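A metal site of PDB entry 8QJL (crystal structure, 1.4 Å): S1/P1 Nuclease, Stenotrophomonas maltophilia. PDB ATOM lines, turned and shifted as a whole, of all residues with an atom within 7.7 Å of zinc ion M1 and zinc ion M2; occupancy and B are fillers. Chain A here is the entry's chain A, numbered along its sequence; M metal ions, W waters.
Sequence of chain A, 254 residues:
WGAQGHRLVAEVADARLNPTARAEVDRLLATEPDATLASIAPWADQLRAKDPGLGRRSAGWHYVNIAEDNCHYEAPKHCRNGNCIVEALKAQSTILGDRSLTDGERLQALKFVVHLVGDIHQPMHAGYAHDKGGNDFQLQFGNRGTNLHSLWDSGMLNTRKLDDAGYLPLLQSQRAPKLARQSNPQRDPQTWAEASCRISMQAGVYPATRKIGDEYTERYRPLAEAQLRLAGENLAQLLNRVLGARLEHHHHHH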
ATOM      1  N   TRP A   1      -1.228  16.295  23.906  1.00  0.00           N
ATOM      2  CA  TRP A   1      -1.351  17.722  23.539  1.00  0.00           C
ATOM      3  C   TRP A   1      -1.606  18.545  24.806  1.00  0.00           C
ATOM      4  O   TRP A   1      -2.099  18.023  25.805  1.00  0.00           O
ATOM      5  CB  TRP A   1      -2.527  17.935  22.611  1.00  0.00           C
ATOM      6  CG  TRP A   1      -2.510  17.079  21.392  1.00  0.00           C
ATOM      7  CD1 TRP A   1      -3.250  15.944  21.214  1.00  0.00           C
ATOM      8  CD2 TRP A   1      -1.739  17.250  20.196  1.00  0.00           C
ATOM      9  NE1 TRP A   1      -2.999  15.404  19.981  1.00  0.00           N
ATOM     10  CE2 TRP A   1      -2.106  16.203  19.332  1.00  0.00           C
ATOM     11  CE3 TRP A   1      -0.789  18.177  19.769  1.00  0.00           C
ATOM     12  CZ2 TRP A   1      -1.540  16.038  18.066  1.00  0.00           C
ATOM     13  CZ3 TRP A   1      -0.242  18.013  18.508  1.00  0.00           C
ATOM     14  CH2 TRP A   1      -0.613  16.971  17.667  1.00  0.00           C
ATOM     15  N   GLY A   2      -1.312  19.827  24.715  1.00  0.00           N
ATOM     16  CA  GLY A   2      -1.869  20.796  25.669  1.00  0.00           C
ATOM     17  C   GLY A   2      -3.351  21.016  25.463  1.00  0.00           C
ATOM     18  O   GLY A   2      -3.995  20.385  24.590  1.00  0.00           O
ATOM     19  N   ALA A   3      -3.919  21.867  26.289  1.00  0.00           N
ATOM     20  CA  ALA A   3      -5.379  21.993  26.379  1.00  0.00           C
ATOM     21  C   ALA A   3      -5.943  22.452  25.047  1.00  0.00           C
ATOM     22  O   ALA A   3      -6.953  21.889  24.612  1.00  0.00           O
ATOM     23  CB  ALA A   3      -5.746  22.887  27.523  1.00  0.00           C
ATOM     24  N   GLY A   5      -4.877  21.982  21.984  1.00  0.00           N
ATOM     25  CA  GLY A   5      -4.903  20.859  21.057  1.00  0.00           C
ATOM     26  C   GLY A   5      -6.040  19.902  21.372  1.00  0.00           C
ATOM     27  O   GLY A   5      -6.759  19.489  20.437  1.00  0.00           O
ATOM     28  N   HIS A   6      -6.260  19.586  22.647  1.00  0.00           N
ATOM     29  CA  HIS A   6      -7.381  18.702  23.045  1.00  0.00           C
ATOM     30  C   HIS A   6      -8.734  19.309  22.648  1.00  0.00           C
ATOM     31  O   HIS A   6      -9.591  18.570  22.130  1.00  0.00           O
ATOM     32  CB  HIS A   6      -7.322  18.366  24.518  1.00  0.00           C
ATOM     33  CG  HIS A   6      -6.293  17.331  24.771  1.00  0.00           C
ATOM     34  ND1 HIS A   6      -6.456  16.029  24.345  1.00  0.00           N
ATOM     35  CD2 HIS A   6      -5.049  17.420  25.297  1.00  0.00           C
ATOM     36  CE1 HIS A   6      -5.323  15.350  24.593  1.00  0.00           C
ATOM     37  NE2 HIS A   6      -4.447  16.190  25.197  1.00  0.00           N
ATOM     38  N   ALA A  41     -12.450  18.209  27.064  1.00  0.00           N
ATOM     39  CA  ALA A  41     -11.333  17.546  26.351  1.00  0.00           C
ATOM     40  C   ALA A  41     -10.029  17.604  27.151  1.00  0.00           C
ATOM     41  O   ALA A  41      -9.262  16.630  27.104  1.00  0.00           O
ATOM     42  CB  ALA A  41     -11.174  18.094  24.945  1.00  0.00           C
ATOM     43  N   PRO A  42      -9.675  18.706  27.836  1.00  0.00           N
ATOM     44  CA  PRO A  42      -8.465  18.754  28.674  1.00  0.00           C
ATOM     45  C   PRO A  42      -8.573  18.133  30.054  1.00  0.00           C
ATOM     46  O   PRO A  42      -7.554  18.033  30.753  1.00  0.00           O
ATOM     47  CB  PRO A  42      -8.213  20.263  28.839  1.00  0.00           C
ATOM     48  CG  PRO A  42      -9.012  20.913  27.746  1.00  0.00           C
ATOM     49  CD  PRO A  42     -10.247  20.059  27.705  1.00  0.00           C
ATOM     50  N   ALA A  44      -8.711  15.298  31.524  1.00  0.00           N
ATOM     51  CA  ALA A  44      -7.876  14.179  32.005  1.00  0.00           C
ATOM     52  C   ALA A  44      -6.472  14.661  32.377  1.00  0.00           C
ATOM     53  O   ALA A  44      -5.774  13.928  33.112  1.00  0.00           O
ATOM     54  CB  ALA A  44      -7.797  13.064  31.001  1.00  0.00           C
ATOM     55  N   ASP A  45      -6.045  15.853  31.913  1.00  0.00           N
ATOM     56  CA  ASP A  45      -4.727  16.407  32.297  1.00  0.00           C
ATOM     57  C   ASP A  45      -4.811  17.311  33.526  1.00  0.00           C
ATOM     58  O   ASP A  45      -3.747  17.786  33.985  1.00  0.00           O
ATOM     59  CB  ASP A  45      -4.146  17.263  31.161  1.00  0.00           C
ATOM     60  CG  ASP A  45      -3.494  16.507  30.004  1.00  0.00           C
ATOM     61  OD1 ASP A  45      -3.290  15.263  30.129  1.00  0.00           O
ATOM     62  OD2 ASP A  45      -3.236  17.191  28.943  1.00  0.00           O
ATOM     63  N   GLN A  46      -6.021  17.592  34.015  1.00  0.00           N
ATOM     64  CA  GLN A  46      -6.267  18.663  34.987  1.00  0.00           C
ATOM     65  C   GLN A  46      -6.796  18.094  36.291  1.00  0.00           C
ATOM     66  O   GLN A  46      -7.286  18.867  37.114  1.00  0.00           O
ATOM     67  CB  GLN A  46      -7.238  19.680  34.369  1.00  0.00           C
ATOM     68  CG  GLN A  46      -6.652  20.347  33.141  1.00  0.00           C
ATOM     69  CD  GLN A  46      -7.486  21.413  32.482  1.00  0.00           C
ATOM     70  OE1 GLN A  46      -8.691  21.528  32.719  1.00  0.00           O
ATOM     71  NE2 GLN A  46      -6.850  22.183  31.612  1.00  0.00           N
ATOM     72  N   SER A  58      -4.470   7.365  36.595  1.00  0.00           N
ATOM     73  CA  SER A  58      -4.653   7.398  35.117  1.00  0.00           C
ATOM     74  C   SER A  58      -3.531   8.130  34.369  1.00  0.00           C
ATOM     75  O   SER A  58      -3.607   8.222  33.162  1.00  0.00           O
ATOM     76  CB  SER A  58      -5.993   7.982  34.772  1.00  0.00           C
ATOM     77  OG  SER A  58      -6.137   9.312  35.208  1.00  0.00           O
ATOM     78  N   ALA A  59      -2.483   8.598  35.044  1.00  0.00           N
ATOM     79  CA  ALA A  59      -1.440   9.400  34.372  1.00  0.00           C
ATOM     80  C   ALA A  59      -0.738   8.597  33.261  1.00  0.00           C
ATOM     81  O   ALA A  59      -0.432   9.157  32.175  1.00  0.00           O
ATOM     82  CB  ALA A  59      -0.446   9.954  35.335  1.00  0.00           C
ATOM     83  N   TRP A  61      -2.030   6.454  31.356  1.00  0.00           N
ATOM     84  CA  TRP A  61      -2.975   6.137  30.251  1.00  0.00           C
ATOM     85  C   TRP A  61      -2.754   7.086  29.066  1.00  0.00           C
ATOM     86  O   TRP A  61      -3.360   6.860  28.045  1.00  0.00           O
ATOM     87  CB  TRP A  61      -4.418   6.243  30.725  1.00  0.00           C
ATOM     88  CG  TRP A  61      -4.800   5.349  31.841  1.00  0.00           C
ATOM     89  CD1 TRP A  61      -4.060   4.399  32.507  1.00  0.00           C
ATOM     90  CD2 TRP A  61      -6.118   5.280  32.395  1.00  0.00           C
ATOM     91  NE1 TRP A  61      -4.828   3.763  33.433  1.00  0.00           N
ATOM     92  CE2 TRP A  61      -6.081   4.305  33.428  1.00  0.00           C
ATOM     93  CE3 TRP A  61      -7.315   5.959  32.141  1.00  0.00           C
ATOM     94  CZ2 TRP A  61      -7.209   3.989  34.174  1.00  0.00           C
ATOM     95  CZ3 TRP A  61      -8.414   5.665  32.912  1.00  0.00           C
ATOM     96  CH2 TRP A  61      -8.367   4.688  33.905  1.00  0.00           C
ATOM     97  N   HIS A  62      -1.951   8.154  29.224  1.00  0.00           N
ATOM     98  CA  HIS A  62      -1.826   9.180  28.166  1.00  0.00           C
ATOM     99  C   HIS A  62      -0.782   8.817  27.107  1.00  0.00           C
ATOM    100  O   HIS A  62      -0.697   9.535  26.126  1.00  0.00           O
ATOM    101  CB  HIS A  62      -1.538  10.552  28.772  1.00  0.00           C
ATOM    102  CG  HIS A  62      -2.605  11.047  29.674  1.00  0.00           C
ATOM    103  ND1 HIS A  62      -3.213  12.300  29.512  1.00  0.00           N
ATOM    104  CD2 HIS A  62      -3.135  10.485  30.779  1.00  0.00           C
ATOM    105  CE1 HIS A  62      -4.076  12.452  30.519  1.00  0.00           C
ATOM    106  NE2 HIS A  62      -4.055  11.359  31.285  1.00  0.00           N
ATOM    107  N   TYR A  63      -0.042   7.724  27.262  1.00  0.00           N
ATOM    108  CA  TYR A  63       1.058   7.438  26.320  1.00  0.00           C
ATOM    109  C   TYR A  63       1.349   5.951  26.279  1.00  0.00           C
ATOM    110  O   TYR A  63       0.802   5.156  27.062  1.00  0.00           O
ATOM    111  CB  TYR A  63       2.297   8.235  26.662  1.00  0.00           C
ATOM    112  CG  TYR A  63       2.796   8.004  28.048  1.00  0.00           C
ATOM    113  CD1 TYR A  63       2.297   8.743  29.119  1.00  0.00           C
ATOM    114  CD2 TYR A  63       3.722   7.002  28.296  1.00  0.00           C
ATOM    115  CE1 TYR A  63       2.734   8.468  30.403  1.00  0.00           C
ATOM    116  CE2 TYR A  63       4.192   6.745  29.582  1.00  0.00           C
ATOM    117  CZ  TYR A  63       3.697   7.479  30.629  1.00  0.00           C
ATOM    118  OH  TYR A  63       4.154   7.224  31.904  1.00  0.00           O
ATOM    119  N   ILE A  85      -1.956   3.973  26.866  1.00  0.00           N
ATOM    120  CA  ILE A  85      -3.084   4.597  26.142  1.00  0.00           C
ATOM    121  C   ILE A  85      -3.825   3.561  25.308  1.00  0.00           C
ATOM    122  O   ILE A  85      -5.014   3.763  25.076  1.00  0.00           O
ATOM    123  CB  ILE A  85      -2.577   5.776  25.314  1.00  0.00           C
ATOM    124  CG1 ILE A  85      -3.737   6.623  24.805  1.00  0.00           C
ATOM    125  CG2 ILE A  85      -1.637   5.352  24.191  1.00  0.00           C
ATOM    126  CD1 ILE A  85      -3.326   8.045  24.457  1.00  0.00           C
ATOM    127  N   HIS A 115     -10.182  12.734  25.411  1.00  0.00           N
ATOM    128  CA  HIS A 115      -8.798  13.121  25.655  1.00  0.00           C
ATOM    129  C   HIS A 115      -7.852  12.158  24.950  1.00  0.00           C
ATOM    130  O   HIS A 115      -6.872  12.579  24.327  1.00  0.00           O
ATOM    131  CB  HIS A 115      -8.505  13.156  27.138  1.00  0.00           C
ATOM    132  CG  HIS A 115      -7.184  13.755  27.448  1.00  0.00           C
ATOM    133  ND1 HIS A 115      -7.038  15.120  27.638  1.00  0.00           N
ATOM    134  CD2 HIS A 115      -5.969  13.185  27.628  1.00  0.00           C
ATOM    135  CE1 HIS A 115      -5.750  15.363  27.905  1.00  0.00           C
ATOM    136  NE2 HIS A 115      -5.065  14.182  27.910  1.00  0.00           N
ATOM    137  N   LEU A 116      -8.073  10.873  25.162  1.00  0.00           N
ATOM    138  CA  LEU A 116      -7.106   9.829  24.756  1.00  0.00           C
ATOM    139  C   LEU A 116      -7.107   9.694  23.219  1.00  0.00           C
ATOM    140  O   LEU A 116      -6.054   9.397  22.650  1.00  0.00           O
ATOM    141  CB  LEU A 116      -7.409   8.506  25.449  1.00  0.00           C
ATOM    142  CG  LEU A 116      -7.192   8.506  26.968  1.00  0.00           C
ATOM    143  CD1 LEU A 116      -7.483   7.143  27.480  1.00  0.00           C
ATOM    144  CD2 LEU A 116      -5.806   8.951  27.361  1.00  0.00           C
ATOM    145  N   GLY A 118      -7.263  12.169  21.350  1.00  0.00           N
ATOM    146  CA  GLY A 118      -6.303  13.260  21.080  1.00  0.00           C
ATOM    147  C   GLY A 118      -4.855  12.808  21.330  1.00  0.00           C
ATOM    148  O   GLY A 118      -4.025  12.846  20.423  1.00  0.00           O
ATOM    149  N   ASP A 119      -4.576  12.308  22.536  1.00  0.00           N
ATOM    150  CA  ASP A 119      -3.185  11.976  22.895  1.00  0.00           C
ATOM    151  C   ASP A 119      -2.619  10.860  22.010  1.00  0.00           C
ATOM    152  O   ASP A 119      -1.400  10.880  21.717  1.00  0.00           O
ATOM    153  CB  ASP A 119      -3.029  11.582  24.356  1.00  0.00           C
ATOM    154  CG  ASP A 119      -2.844  12.774  25.284  1.00  0.00           C
ATOM    155  OD1 ASP A 119      -2.645  13.885  24.797  1.00  0.00           O
ATOM    156  OD2 ASP A 119      -2.906  12.545  26.548  1.00  0.00           O
ATOM    157  N   ILE A 120      -3.412   9.899  21.550  1.00  0.00           N
ATOM    158  CA  ILE A 120      -2.873   8.745  20.806  1.00  0.00           C
ATOM    159  C   ILE A 120      -2.485   9.171  19.396  1.00  0.00           C
ATOM    160  O   ILE A 120      -1.819   8.395  18.727  1.00  0.00           O
ATOM    161  CB  ILE A 120      -3.873   7.571  20.829  1.00  0.00           C
ATOM    162  CG1 ILE A 120      -3.196   6.228  20.610  1.00  0.00           C
ATOM    163  CG2 ILE A 120      -5.035   7.749  19.883  1.00  0.00           C
ATOM    164  CD1 ILE A 120      -4.078   5.025  20.967  1.00  0.00           C
ATOM    165  N   GLN A 122      -0.801  12.172  19.060  1.00  0.00           N
ATOM    166  CA  GLN A 122       0.370  13.049  19.284  1.00  0.00           C
ATOM    167  C   GLN A 122       1.580  12.146  19.136  1.00  0.00           C
ATOM    168  O   GLN A 122       1.786  11.279  19.996  1.00  0.00           O
ATOM    169  CB  GLN A 122       0.278  13.689  20.663  1.00  0.00           C
ATOM    170  CG  GLN A 122       0.972  15.036  20.851  1.00  0.00           C
ATOM    171  CD  GLN A 122       2.480  15.037  20.792  1.00  0.00           C
ATOM    172  OE1 GLN A 122       3.089  14.528  19.850  1.00  0.00           O
ATOM    173  NE2 GLN A 122       3.119  15.604  21.818  1.00  0.00           N
ATOM    174  N   HIS A 125       3.620  11.035  22.163  1.00  0.00           N
ATOM    175  CA  HIS A 125       2.904  10.194  23.137  1.00  0.00           C
ATOM    176  C   HIS A 125       3.010   8.709  22.752  1.00  0.00           C
ATOM    177  O   HIS A 125       2.461   7.886  23.531  1.00  0.00           O
ATOM    178  CB  HIS A 125       1.448  10.625  23.292  1.00  0.00           C
ATOM    179  CG  HIS A 125       1.258  11.820  24.168  1.00  0.00           C
ATOM    180  ND1 HIS A 125       0.511  11.754  25.315  1.00  0.00           N
ATOM    181  CD2 HIS A 125       1.786  13.089  24.104  1.00  0.00           C
ATOM    182  CE1 HIS A 125       0.571  12.939  25.926  1.00  0.00           C
ATOM    183  NE2 HIS A 125       1.381  13.767  25.230  1.00  0.00           N
ATOM    184  N   HIS A 149       9.091  16.816  23.298  1.00  0.00           N
ATOM    185  CA  HIS A 149       7.724  16.428  23.708  1.00  0.00           C
ATOM    186  C   HIS A 149       6.833  17.678  23.766  1.00  0.00           C
ATOM    187  O   HIS A 149       5.779  17.726  23.104  1.00  0.00           O
ATOM    188  CB  HIS A 149       7.738  15.681  25.029  1.00  0.00           C
ATOM    189  CG  HIS A 149       6.406  15.094  25.344  1.00  0.00           C
ATOM    190  ND1 HIS A 149       6.056  13.812  25.065  1.00  0.00           N
ATOM    191  CD2 HIS A 149       5.300  15.728  25.754  1.00  0.00           C
ATOM    192  CE1 HIS A 149       4.759  13.655  25.370  1.00  0.00           C
ATOM    193  NE2 HIS A 149       4.264  14.839  25.767  1.00  0.00           N
ATOM    194  N   ASP A 153       3.490  18.959  21.883  1.00  0.00           N
ATOM    195  CA  ASP A 153       2.260  19.135  22.676  1.00  0.00           C
ATOM    196  C   ASP A 153       1.659  20.514  22.431  1.00  0.00           C
ATOM    197  O   ASP A 153       0.407  20.603  22.381  1.00  0.00           O
ATOM    198  CB  ASP A 153       2.462  18.974  24.180  1.00  0.00           C
ATOM    199  CG  ASP A 153       2.288  17.569  24.752  1.00  0.00           C
ATOM    200  OD1 ASP A 153       1.789  16.676  24.057  1.00  0.00           O
ATOM    201  OD2 ASP A 153       2.731  17.382  25.916  1.00  0.00           O
HETATM  202 ZN    ZN M   1      -3.008  13.804  28.173  1.00  0.00          ZN
HETATM  203 ZN    ZN M   2      -2.500  15.816  25.555  1.00  0.00          ZN
HETATM  204 ZN    ZN M   3       2.284  15.402  26.181  1.00  0.00          ZN
HETATM  205  O   HOH W   1      -0.646  13.641  29.029  1.00  0.00           O
HETATM  206  O   HOH W   2       0.437  16.113  26.866  1.00  0.00           O
HETATM  207  O   HOH W   3      -2.094  15.359  27.386  1.00  0.00           O
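ND1 of His 6 sits at hydrogen-bond distance from ND1 of His 115. ND1 of His 125 is in hydrogen-bond range of O of His 62. A ring nitrogen (ND1) of His 115 is in hydrogen-bond range of the backbone carbonyl oxygen (O) of Ala 41 (2.7 Å). The indole nitrogen (NE1) of Trp 1 lies within hydrogen-bond range of the backbone carbonyl oxygen (O) of Gly 118, 2.8 Å away.
Within 4 Å of zinc ion M1: Asp 45, His 62, His 115 and Asp 119. The nearest printed residue that does not touch zinc ion M1 is His 6 (4.1 Å).
Of the 25 residues printed, 5 come within 4 Å of zinc ion M2.
Water W3 is bound to zinc ion M1, at 2.0 Å. Zinc ion M1 is bound by ND1 of His 62 (2.0 Å). OD2 of Asp 119 is bound to zinc ion M1. NE2 of His 115 binds zinc ion M1. Zinc ion M1 is bound by OD1 of Asp 45, 2.5 Å away. Water W1 is bound to zinc ion M1. Zinc ion M1 has six donor atoms within binding distance.
Zinc ion M2 is bound by water W3 (1.9 Å), NE2 of His 6 (2.0 Å), OD1 of Asp 119 (2.1 Å), N of Trp 1 (2.1 Å) and O of Trp 1 (2.3 Å). Zinc ion M2 has five donor atoms within binding distance.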
